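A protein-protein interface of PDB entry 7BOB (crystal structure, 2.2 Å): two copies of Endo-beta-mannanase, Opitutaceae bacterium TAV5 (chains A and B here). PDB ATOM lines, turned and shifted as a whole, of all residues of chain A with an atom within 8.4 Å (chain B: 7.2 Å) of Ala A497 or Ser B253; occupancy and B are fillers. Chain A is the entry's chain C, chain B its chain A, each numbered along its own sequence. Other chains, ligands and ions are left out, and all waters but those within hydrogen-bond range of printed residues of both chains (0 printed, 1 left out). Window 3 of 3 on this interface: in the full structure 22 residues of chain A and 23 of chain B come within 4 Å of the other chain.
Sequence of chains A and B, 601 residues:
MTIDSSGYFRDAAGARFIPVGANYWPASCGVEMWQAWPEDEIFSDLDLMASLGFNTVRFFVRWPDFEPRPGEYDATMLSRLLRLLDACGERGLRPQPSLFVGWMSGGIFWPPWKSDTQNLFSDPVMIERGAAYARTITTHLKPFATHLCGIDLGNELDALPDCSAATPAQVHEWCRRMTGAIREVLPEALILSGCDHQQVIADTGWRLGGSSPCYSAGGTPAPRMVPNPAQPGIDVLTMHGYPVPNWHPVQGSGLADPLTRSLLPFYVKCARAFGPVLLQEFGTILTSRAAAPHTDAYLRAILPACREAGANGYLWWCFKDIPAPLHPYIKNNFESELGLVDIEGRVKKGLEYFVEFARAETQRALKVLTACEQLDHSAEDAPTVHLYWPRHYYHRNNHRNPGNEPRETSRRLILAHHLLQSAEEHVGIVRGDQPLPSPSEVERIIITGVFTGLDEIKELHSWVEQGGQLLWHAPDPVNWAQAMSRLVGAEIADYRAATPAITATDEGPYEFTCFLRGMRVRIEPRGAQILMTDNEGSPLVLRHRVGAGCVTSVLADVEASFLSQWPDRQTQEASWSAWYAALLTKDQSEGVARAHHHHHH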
ATOM      1  N   ASP A 494      -1.278 -27.116   2.875  1.00  0.00           N
ATOM      2  CA  ASP A 494      -0.884 -25.941   2.107  1.00  0.00           C
ATOM      3  C   ASP A 494      -2.032 -24.937   2.177  1.00  0.00           C
ATOM      4  O   ASP A 494      -3.159 -25.294   2.533  1.00  0.00           O
ATOM      5  CB  ASP A 494      -0.571 -26.293   0.634  1.00  0.00           C
ATOM      6  CG  ASP A 494       0.226 -25.207  -0.077  1.00  0.00           C
ATOM      7  OD1 ASP A 494       0.632 -24.227   0.597  1.00  0.00           O
ATOM      8  OD2 ASP A 494       0.455 -25.338  -1.309  1.00  0.00           O
ATOM      9  N   TYR A 495      -1.732 -23.684   1.843  1.00  0.00           N
ATOM     10  CA  TYR A 495      -2.792 -22.764   1.466  1.00  0.00           C
ATOM     11  C   TYR A 495      -3.252 -23.090   0.042  1.00  0.00           C
ATOM     12  O   TYR A 495      -2.589 -23.822  -0.697  1.00  0.00           O
ATOM     13  CB  TYR A 495      -2.315 -21.310   1.540  1.00  0.00           C
ATOM     14  CG  TYR A 495      -1.622 -20.941   2.835  1.00  0.00           C
ATOM     15  CD1 TYR A 495      -2.353 -20.565   3.954  1.00  0.00           C
ATOM     16  CD2 TYR A 495      -0.231 -20.982   2.940  1.00  0.00           C
ATOM     17  CE1 TYR A 495      -1.717 -20.221   5.140  1.00  0.00           C
ATOM     18  CE2 TYR A 495       0.418 -20.652   4.131  1.00  0.00           C
ATOM     19  CZ  TYR A 495      -0.332 -20.268   5.223  1.00  0.00           C
ATOM     20  OH  TYR A 495       0.293 -19.935   6.410  1.00  0.00           O
ATOM     21  N   ARG A 496      -4.408 -22.548  -0.330  1.00  0.00           N
ATOM     22  CA  ARG A 496      -4.905 -22.618  -1.696  1.00  0.00           C
ATOM     23  C   ARG A 496      -5.554 -21.282  -1.998  1.00  0.00           C
ATOM     24  O   ARG A 496      -5.821 -20.496  -1.090  1.00  0.00           O
ATOM     25  CB  ARG A 496      -5.906 -23.765  -1.896  1.00  0.00           C
ATOM     26  CG  ARG A 496      -6.964 -23.881  -0.793  1.00  0.00           C
ATOM     27  CD  ARG A 496      -8.191 -24.609  -1.303  1.00  0.00           C
ATOM     28  NE  ARG A 496      -8.690 -23.944  -2.498  1.00  0.00           N
ATOM     29  CZ  ARG A 496      -9.336 -24.554  -3.492  1.00  0.00           C
ATOM     30  NH1 ARG A 496      -9.567 -25.866  -3.430  1.00  0.00           N
ATOM     31  NH2 ARG A 496      -9.750 -23.848  -4.543  1.00  0.00           N
ATOM     32  N   ALA A 497      -5.790 -21.022  -3.285  1.00  0.00           N
ATOM     33  CA  ALA A 497      -6.464 -19.801  -3.709  1.00  0.00           C
ATOM     34  C   ALA A 497      -7.793 -19.641  -2.981  1.00  0.00           C
ATOM     35  O   ALA A 497      -8.539 -20.608  -2.808  1.00  0.00           O
ATOM     36  CB  ALA A 497      -6.694 -19.825  -5.228  1.00  0.00           C
ATOM     37  N   ALA A 498      -8.076 -18.415  -2.528  1.00  0.00           N
ATOM     38  CA  ALA A 498      -9.336 -18.152  -1.834  1.00  0.00           C
ATOM     39  C   ALA A 498     -10.463 -17.899  -2.828  1.00  0.00           C
ATOM     40  O   ALA A 498     -11.147 -16.873  -2.760  1.00  0.00           O
ATOM     41  CB  ALA A 498      -9.202 -16.958  -0.877  1.00  0.00           C
ATOM     42  N   THR A 499     -10.649 -18.816  -3.758  1.00  0.00           N
ATOM     43  CA  THR A 499     -11.713 -18.767  -4.743  1.00  0.00           C
ATOM     44  C   THR A 499     -12.946 -19.470  -4.191  1.00  0.00           C
ATOM     45  O   THR A 499     -12.852 -20.228  -3.215  1.00  0.00           O
ATOM     46  CB  THR A 499     -11.244 -19.406  -6.054  1.00  0.00           C
ATOM     47  OG1 THR A 499     -10.722 -20.718  -5.805  1.00  0.00           O
ATOM     48  CG2 THR A 499     -10.172 -18.537  -6.679  1.00  0.00           C
ATOM     49  N   PRO A 500     -14.127 -19.207  -4.764  1.00  0.00           N
ATOM     50  CA  PRO A 500     -15.361 -19.734  -4.165  1.00  0.00           C
ATOM     51  C   PRO A 500     -15.402 -21.254  -4.158  1.00  0.00           C
ATOM     52  O   PRO A 500     -14.878 -21.923  -5.052  1.00  0.00           O
ATOM     53  CB  PRO A 500     -16.467 -19.147  -5.052  1.00  0.00           C
ATOM     54  CG  PRO A 500     -15.864 -17.898  -5.585  1.00  0.00           C
ATOM     55  CD  PRO A 500     -14.415 -18.240  -5.837  1.00  0.00           C
ATOM     56  N   ALA A 501     -16.029 -21.786  -3.112  1.00  0.00           N
ATOM     57  CA  ALA A 501     -16.271 -23.210  -2.945  1.00  0.00           C
ATOM     58  C   ALA A 501     -17.740 -23.490  -3.244  1.00  0.00           C
ATOM     59  O   ALA A 501     -18.631 -22.923  -2.596  1.00  0.00           O
ATOM     60  CB  ALA A 501     -15.921 -23.659  -1.527  1.00  0.00           C
ATOM     61  N   PHE A 515     -13.935 -16.638   3.288  1.00  0.00           N
ATOM     62  CA  PHE A 515     -13.187 -17.568   4.116  1.00  0.00           C
ATOM     63  C   PHE A 515     -12.501 -16.797   5.230  1.00  0.00           C
ATOM     64  O   PHE A 515     -12.266 -15.589   5.112  1.00  0.00           O
ATOM     65  CB  PHE A 515     -12.194 -18.361   3.260  1.00  0.00           C
ATOM     66  CG  PHE A 515     -12.862 -19.113   2.155  1.00  0.00           C
ATOM     67  CD1 PHE A 515     -13.160 -18.478   0.954  1.00  0.00           C
ATOM     68  CD2 PHE A 515     -13.259 -20.430   2.335  1.00  0.00           C
ATOM     69  CE1 PHE A 515     -13.812 -19.149  -0.071  1.00  0.00           C
ATOM     70  CE2 PHE A 515     -13.904 -21.118   1.312  1.00  0.00           C
ATOM     71  CZ  PHE A 515     -14.183 -20.473   0.105  1.00  0.00           C
ATOM     72  N   GLY A 518      -9.839 -14.208   4.899  1.00  0.00           N
ATOM     73  CA  GLY A 518      -9.649 -14.186   3.467  1.00  0.00           C
ATOM     74  C   GLY A 518      -8.606 -15.162   2.973  1.00  0.00           C
ATOM     75  O   GLY A 518      -7.878 -14.840   2.036  1.00  0.00           O
ATOM     76  N   MET A 519      -8.492 -16.334   3.605  1.00  0.00           N
ATOM     77  CA  MET A 519      -7.558 -17.376   3.199  1.00  0.00           C
ATOM     78  C   MET A 519      -8.260 -18.721   3.234  1.00  0.00           C
ATOM     79  O   MET A 519      -9.128 -18.970   4.076  1.00  0.00           O
ATOM     80  CB  MET A 519      -6.315 -17.434   4.107  1.00  0.00           C
ATOM     81  CG  MET A 519      -5.445 -16.191   4.045  1.00  0.00           C
ATOM     82  SD  MET A 519      -3.795 -16.403   4.761  1.00  0.00           S
ATOM     83  CE  MET A 519      -4.240 -16.600   6.480  1.00  0.00           C
ATOM     84  N   ARG A 520      -7.864 -19.587   2.312  1.00  0.00           N
ATOM     85  CA  ARG A 520      -8.314 -20.968   2.258  1.00  0.00           C
ATOM     86  C   ARG A 520      -7.113 -21.867   2.486  1.00  0.00           C
ATOM     87  O   ARG A 520      -5.997 -21.536   2.083  1.00  0.00           O
ATOM     88  CB  ARG A 520      -8.943 -21.307   0.905  1.00  0.00           C
ATOM     89  CG  ARG A 520     -10.431 -21.364   0.915  1.00  0.00           C
ATOM     90  CD  ARG A 520     -10.957 -21.750  -0.452  1.00  0.00           C
ATOM     91  NE  ARG A 520     -11.477 -23.113  -0.469  1.00  0.00           N
ATOM     92  CZ  ARG A 520     -12.041 -23.676  -1.532  1.00  0.00           C
ATOM     93  NH1 ARG A 520     -12.153 -22.991  -2.661  1.00  0.00           N
ATOM     94  NH2 ARG A 520     -12.488 -24.924  -1.469  1.00  0.00           N
ATOM     95  N   VAL A 521      -7.348 -23.007   3.125  1.00  0.00           N
ATOM     96  CA  VAL A 521      -6.289 -23.985   3.337  1.00  0.00           C
ATOM     97  C   VAL A 521      -6.678 -25.303   2.690  1.00  0.00           C
ATOM     98  O   VAL A 521      -7.850 -25.680   2.637  1.00  0.00           O
ATOM     99  CB  VAL A 521      -5.975 -24.206   4.831  1.00  0.00           C
ATOM    100  CG1 VAL A 521      -5.255 -22.995   5.403  1.00  0.00           C
ATOM    101  CG2 VAL A 521      -7.251 -24.527   5.620  1.00  0.00           C
ATOM    102  N   ARG A 522      -5.670 -26.008   2.203  1.00  0.00           N
ATOM    103  CA  ARG A 522      -5.806 -27.396   1.789  1.00  0.00           C
ATOM    104  C   ARG A 522      -5.488 -28.293   2.979  1.00  0.00           C
ATOM    105  O   ARG A 522      -4.416 -28.169   3.582  1.00  0.00           O
ATOM    106  CB  ARG A 522      -4.862 -27.675   0.629  1.00  0.00           C
ATOM    107  CG  ARG A 522      -5.201 -28.930  -0.119  1.00  0.00           C
ATOM    108  CD  ARG A 522      -4.526 -28.984  -1.492  1.00  0.00           C
ATOM    109  NE  ARG A 522      -5.029 -28.014  -2.472  1.00  0.00           N
ATOM    110  CZ  ARG A 522      -6.217 -28.076  -3.079  1.00  0.00           C
ATOM    111  NH1 ARG A 522      -7.078 -29.052  -2.786  1.00  0.00           N
ATOM    112  NH2 ARG A 522      -6.549 -27.152  -3.979  1.00  0.00           N
ATOM    113  N   ASP A 534     -15.996 -29.896  -2.138  1.00  0.00           N
ATOM    114  CA  ASP A 534     -16.452 -28.906  -3.094  1.00  0.00           C
ATOM    115  C   ASP A 534     -16.542 -29.554  -4.478  1.00  0.00           C
ATOM    116  O   ASP A 534     -16.124 -30.699  -4.688  1.00  0.00           O
ATOM    117  CB  ASP A 534     -15.552 -27.667  -3.082  1.00  0.00           C
ATOM    118  CG  ASP A 534     -14.163 -27.926  -3.623  1.00  0.00           C
ATOM    119  OD1 ASP A 534     -13.700 -29.091  -3.585  1.00  0.00           O
ATOM    120  OD2 ASP A 534     -13.537 -26.945  -4.093  1.00  0.00           O
ATOM    121  N   GLU A 536     -14.869 -29.384  -6.913  1.00  0.00           N
ATOM    122  CA  GLU A 536     -13.565 -29.714  -7.467  1.00  0.00           C
ATOM    123  C   GLU A 536     -12.874 -30.829  -6.699  1.00  0.00           C
ATOM    124  O   GLU A 536     -11.681 -31.058  -6.907  1.00  0.00           O
ATOM    125  CB  GLU A 536     -12.665 -28.482  -7.501  1.00  0.00           C
ATOM    126  CG  GLU A 536     -12.887 -27.591  -8.698  1.00  0.00           C
ATOM    127  CD  GLU A 536     -12.405 -26.177  -8.439  1.00  0.00           C
ATOM    128  OE1 GLU A 536     -13.003 -25.234  -9.009  1.00  0.00           O
ATOM    129  OE2 GLU A 536     -11.432 -26.011  -7.661  1.00  0.00           O
ATOM    130  N   PRO B 243       5.298 -17.224   3.399  1.00  0.00           N
ATOM    131  CA  PRO B 243       4.341 -17.440   2.292  1.00  0.00           C
ATOM    132  C   PRO B 243       2.867 -17.177   2.602  1.00  0.00           C
ATOM    133  O   PRO B 243       2.043 -17.311   1.692  1.00  0.00           O
ATOM    134  CB  PRO B 243       4.554 -18.925   1.962  1.00  0.00           C
ATOM    135  CG  PRO B 243       4.996 -19.554   3.281  1.00  0.00           C
ATOM    136  CD  PRO B 243       5.794 -18.488   3.984  1.00  0.00           C
ATOM    137  N   PRO B 245      -0.609 -16.034   2.557  1.00  0.00           N
ATOM    138  CA  PRO B 245      -1.157 -15.160   1.505  1.00  0.00           C
ATOM    139  C   PRO B 245      -1.545 -13.765   1.986  1.00  0.00           C
ATOM    140  O   PRO B 245      -1.215 -12.784   1.309  1.00  0.00           O
ATOM    141  CB  PRO B 245      -2.360 -15.963   0.994  1.00  0.00           C
ATOM    142  CG  PRO B 245      -1.947 -17.371   1.180  1.00  0.00           C
ATOM    143  CD  PRO B 245      -1.186 -17.389   2.502  1.00  0.00           C
ATOM    144  N   VAL B 250      -0.340  -8.514  -2.594  1.00  0.00           N
ATOM    145  CA  VAL B 250      -0.894  -9.352  -3.653  1.00  0.00           C
ATOM    146  C   VAL B 250      -1.085 -10.744  -3.072  1.00  0.00           C
ATOM    147  O   VAL B 250      -0.148 -11.316  -2.512  1.00  0.00           O
ATOM    148  CB  VAL B 250       0.021  -9.407  -4.888  1.00  0.00           C
ATOM    149  CG1 VAL B 250      -0.639 -10.233  -5.990  1.00  0.00           C
ATOM    150  CG2 VAL B 250       0.353  -8.003  -5.369  1.00  0.00           C
ATOM    151  N   GLN B 251      -2.276 -11.293  -3.221  1.00  0.00           N
ATOM    152  CA  GLN B 251      -2.650 -12.537  -2.550  1.00  0.00           C
ATOM    153  C   GLN B 251      -2.239 -13.736  -3.409  1.00  0.00           C
ATOM    154  O   GLN B 251      -2.907 -14.069  -4.393  1.00  0.00           O
ATOM    155  CB  GLN B 251      -4.149 -12.530  -2.282  1.00  0.00           C
ATOM    156  CG  GLN B 251      -4.588 -13.404  -1.151  1.00  0.00           C
ATOM    157  CD  GLN B 251      -4.760 -12.627   0.111  1.00  0.00           C
ATOM    158  OE1 GLN B 251      -4.369 -11.451   0.185  1.00  0.00           O
ATOM    159  NE2 GLN B 251      -5.325 -13.268   1.136  1.00  0.00           N
ATOM    160  N   GLY B 252      -1.134 -14.392  -3.047  1.00  0.00           N
ATOM    161  CA  GLY B 252      -0.769 -15.643  -3.677  1.00  0.00           C
ATOM    162  C   GLY B 252      -1.567 -16.807  -3.121  1.00  0.00           C
ATOM    163  O   GLY B 252      -2.433 -16.654  -2.264  1.00  0.00           O
ATOM    164  N   SER B 253      -1.247 -18.007  -3.600  1.00  0.00           N
ATOM    165  CA  SER B 253      -2.000 -19.203  -3.238  1.00  0.00           C
ATOM    166  C   SER B 253      -1.215 -20.205  -2.404  1.00  0.00           C
ATOM    167  O   SER B 253      -1.749 -21.275  -2.090  1.00  0.00           O
ATOM    168  CB  SER B 253      -2.565 -19.882  -4.489  1.00  0.00           C
ATOM    169  OG  SER B 253      -3.255 -18.927  -5.283  1.00  0.00           O
ATOM    170  N   GLY B 254       0.010 -19.878  -2.000  1.00  0.00           N
ATOM    171  CA  GLY B 254       0.710 -20.714  -1.040  1.00  0.00           C
ATOM    172  C   GLY B 254       1.994 -21.352  -1.530  1.00  0.00           C
ATOM    173  O   GLY B 254       2.626 -20.868  -2.473  1.00  0.00           O
ATOM    174  N   LEU B 255       2.381 -22.451  -0.885  1.00  0.00           N
ATOM    175  CA  LEU B 255       3.728 -22.989  -1.053  1.00  0.00           C
ATOM    176  C   LEU B 255       4.005 -23.389  -2.502  1.00  0.00           C
ATOM    177  O   LEU B 255       5.110 -23.169  -3.014  1.00  0.00           O
ATOM    178  CB  LEU B 255       3.920 -24.180  -0.131  1.00  0.00           C
ATOM    179  CG  LEU B 255       3.918 -23.807   1.342  1.00  0.00           C
ATOM    180  CD1 LEU B 255       3.668 -25.037   2.195  1.00  0.00           C
ATOM    181  CD2 LEU B 255       5.215 -23.114   1.706  1.00  0.00           C
ATOM    182  N   ALA B 256       3.007 -23.950  -3.186  1.00  0.00           N
ATOM    183  CA  ALA B 256       3.188 -24.402  -4.568  1.00  0.00           C
ATOM    184  C   ALA B 256       3.012 -23.292  -5.601  1.00  0.00           C
ATOM    185  O   ALA B 256       3.293 -23.526  -6.783  1.00  0.00           O
ATOM    186  CB  ALA B 256       2.206 -25.536  -4.890  1.00  0.00           C
ATOM    187  N   ASP B 257       2.551 -22.099  -5.198  1.00  0.00           N
ATOM    188  CA  ASP B 257       2.256 -21.037  -6.161  1.00  0.00           C
ATOM    189  C   ASP B 257       3.531 -20.314  -6.576  1.00  0.00           C
ATOM    190  O   ASP B 257       4.243 -19.793  -5.713  1.00  0.00           O
ATOM    191  CB  ASP B 257       1.261 -20.040  -5.554  1.00  0.00           C
ATOM    192  CG  ASP B 257       0.869 -18.916  -6.520  1.00  0.00           C
ATOM    193  OD1 ASP B 257       1.258 -18.940  -7.715  1.00  0.00           O
ATOM    194  OD2 ASP B 257       0.176 -17.988  -6.072  1.00  0.00           O
ATOM    195  N   PRO B 258       3.848 -20.253  -7.867  1.00  0.00           N
ATOM    196  CA  PRO B 258       4.966 -19.398  -8.321  1.00  0.00           C
ATOM    197  C   PRO B 258       4.861 -17.918  -7.903  1.00  0.00           C
ATOM    198  O   PRO B 258       5.903 -17.276  -7.696  1.00  0.00           O
ATOM    199  CB  PRO B 258       4.909 -19.538  -9.852  1.00  0.00           C
ATOM    200  CG  PRO B 258       4.196 -20.838 -10.097  1.00  0.00           C
ATOM    201  CD  PRO B 258       3.256 -21.056  -8.956  1.00  0.00           C
ATOM    202  N   LEU B 259       3.653 -17.334  -7.832  1.00  0.00           N
ATOM    203  CA  LEU B 259       3.526 -15.967  -7.300  1.00  0.00           C
ATOM    204  C   LEU B 259       4.046 -15.889  -5.867  1.00  0.00           C
ATOM    205  O   LEU B 259       4.941 -15.094  -5.561  1.00  0.00           O
ATOM    206  CB  LEU B 259       2.070 -15.473  -7.364  1.00  0.00           C
ATOM    207  CG  LEU B 259       1.747 -14.008  -6.941  1.00  0.00           C
ATOM    208  CD1 LEU B 259       1.651 -13.816  -5.409  1.00  0.00           C
ATOM    209  CD2 LEU B 259       2.744 -12.998  -7.492  1.00  0.00           C
ATOM    210  N   THR B 260       3.485 -16.705  -4.973  1.00  0.00           N
ATOM    211  CA  THR B 260       3.957 -16.741  -3.594  1.00  0.00           C
ATOM    212  C   THR B 260       5.472 -16.943  -3.536  1.00  0.00           C
ATOM    213  O   THR B 260       6.177 -16.215  -2.823  1.00  0.00           O
ATOM    214  CB  THR B 260       3.257 -17.857  -2.813  1.00  0.00           C
ATOM    215  OG1 THR B 260       1.839 -17.659  -2.822  1.00  0.00           O
ATOM    216  CG2 THR B 260       3.756 -17.901  -1.358  1.00  0.00           C
ATOM    217  N   TRP B 566      -8.262 -10.353 -10.395  1.00  0.00           N
ATOM    218  CA  TRP B 566      -7.647 -11.419  -9.615  1.00  0.00           C
ATOM    219  C   TRP B 566      -8.498 -12.675  -9.454  1.00  0.00           C
ATOM    220  O   TRP B 566      -7.923 -13.780  -9.505  1.00  0.00           O
ATOM    221  CB  TRP B 566      -7.245 -10.887  -8.236  1.00  0.00           C
ATOM    222  CG  TRP B 566      -6.098 -11.653  -7.654  1.00  0.00           C
ATOM    223  CD1 TRP B 566      -6.117 -12.445  -6.542  1.00  0.00           C
ATOM    224  CD2 TRP B 566      -4.774 -11.738  -8.186  1.00  0.00           C
ATOM    225  NE1 TRP B 566      -4.875 -12.992  -6.332  1.00  0.00           N
ATOM    226  CE2 TRP B 566      -4.034 -12.576  -7.335  1.00  0.00           C
ATOM    227  CE3 TRP B 566      -4.135 -11.166  -9.292  1.00  0.00           C
ATOM    228  CZ2 TRP B 566      -2.693 -12.867  -7.561  1.00  0.00           C
ATOM    229  CZ3 TRP B 566      -2.812 -11.450  -9.510  1.00  0.00           C
ATOM    230  CH2 TRP B 566      -2.098 -12.293  -8.649  1.00  0.00           C
ATOM    231  N   ARG B 569      -7.801 -15.297 -11.983  1.00  0.00           N
ATOM    232  CA  ARG B 569      -6.361 -15.461 -12.170  1.00  0.00           C
ATOM    233  C   ARG B 569      -5.999 -16.740 -12.934  1.00  0.00           C
ATOM    234  O   ARG B 569      -5.132 -16.726 -13.825  1.00  0.00           O
ATOM    235  CB  ARG B 569      -5.700 -15.456 -10.791  1.00  0.00           C
ATOM    236  CG  ARG B 569      -4.214 -15.455 -10.823  1.00  0.00           C
ATOM    237  CD  ARG B 569      -3.592 -15.845  -9.478  1.00  0.00           C
ATOM    238  NE  ARG B 569      -2.243 -16.320  -9.754  1.00  0.00           N
ATOM    239  CZ  ARG B 569      -1.429 -16.928  -8.898  1.00  0.00           C
ATOM    240  NH1 ARG B 569      -1.792 -17.152  -7.638  1.00  0.00           N
ATOM    241  NH2 ARG B 569      -0.231 -17.310  -9.328  1.00  0.00           N
ATOM    242  N   GLN B 570      -6.625 -17.864 -12.564  1.00  0.00           N
ATOM    243  CA  GLN B 570      -6.292 -19.160 -13.148  1.00  0.00           C
ATOM    244  C   GLN B 570      -6.289 -19.106 -14.668  1.00  0.00           C
ATOM    245  O   GLN B 570      -5.306 -19.479 -15.318  1.00  0.00           O
ATOM    246  CB  GLN B 570      -7.289 -20.212 -12.665  1.00  0.00           C
ATOM    247  CG  GLN B 570      -6.858 -20.955 -11.421  1.00  0.00           C
ATOM    248  CD  GLN B 570      -7.139 -22.438 -11.521  1.00  0.00           C
ATOM    249  OE1 GLN B 570      -8.162 -22.925 -11.032  1.00  0.00           O
ATOM    250  NE2 GLN B 570      -6.242 -23.166 -12.179  1.00  0.00           N
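The backbone carbonyl oxygen (O) of Asp A494 lies within hydrogen-bond range of the backbone NH (N) of Arg A522 (2.6 Å). The backbone NH (N) of Gly B254 is in hydrogen-bond range of the side-chain hydroxyl (OG1) of Thr B260 (3.0 Å). The backbone NH (N) of Ser B253 lies within hydrogen-bond range of the side-chain hydroxyl (OG1) of Thr B260 (3.2 Å). O of Gln B251 sits at hydrogen-bond distance from NE1 of Trp B566, 3.0 Å away. N of Ser B253 is in hydrogen-bond range of OD2 of Asp B257 (2.9 Å). The backbone NH (N) of Arg A496 sits at hydrogen-bond distance from the backbone carbonyl oxygen (O) of Arg A520, 3.1 Å away.
Asp A494 touches Gly B254 (OD1 to C, 3.8 Å). Tyr A495 touches Pro B245 (CG to CD, 3.6 Å). Ser B253 touches Ala A497. Met A519 touches Pro B245 (SD to CD, 3.6 Å).
Hydrophobic or aromatic side chains of chain A that line the printed part of chain B: Tyr A495, Ala A497 and Met A519. Along chain A the printed residues that touch a printed residue of chain B span positions 494 to 519. Of the 16 printed residues of chain B, 6 touch a printed residue of chain A. Hydrophobic or aromatic side chains of chain B within 4 Å of the printed part of chain A: Pro B245, Leu B255 and Ala B256. Among the printed residues, 9 pairs touch across the chains. Among the printed residues, no Asp or Glu carboxylate lies within 4 Å of a Lys or Arg side-chain nitrogen of the other chain.
No position is printed for both chains. Of the 9 pairs that touch across the chains among the printed residues, none has its exchanged pair printed and touching as well.
The backbone carbonyl oxygen of Ser B253 lies close to the backbone carbonyl oxygen of Tyr A495 (3.0 Å). The backbone carbonyl oxygen (O) of Gly A518 sits at hydrogen-bond distance from the side-chain amide nitrogen (NE2) of Gln B251, 3.1 Å away. The side-chain carboxylate of Asp A494 lies within hydrogen-bond range of the backbone NH of Leu B255. The side-chain carboxylate (OD2) of Asp A494 lies within hydrogen-bond range of the backbone NH (N) of Ala B256 (3.5 Å). N of Arg A496 is in hydrogen-bond range of O of Ser B253 (3.4 Å).
Ala A497 touches just one residue of chain B: Ser B253 (3.6 Å). Of chain A, only Tyr A495, Arg A496 and Ala A497 come within 4 Å of Ser B253. No residue of chain A comes within 4 Å of Gly B252. Gly B254 touches just one residue of chain A: Asp A494. Of the printed residues of chain B, Arg A496 touches Ser B253 (3.4 Å). Of the printed residues of chain A, Leu B255 touches Asp A494. Of the printed residues of chain A, Pro B245 touches Tyr A495 and Met A519. Printed residues of chain B within 4 Å of Met A519: Pro B245. Of the printed residues of chain B, Asp A494 touches Gly B254, Leu B255 and Ala B256. Asp B257 touches none of the printed residues of chain A. The nearest residue of chain B that does not touch Ala A497 is Gly B252 (5.3 Å).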
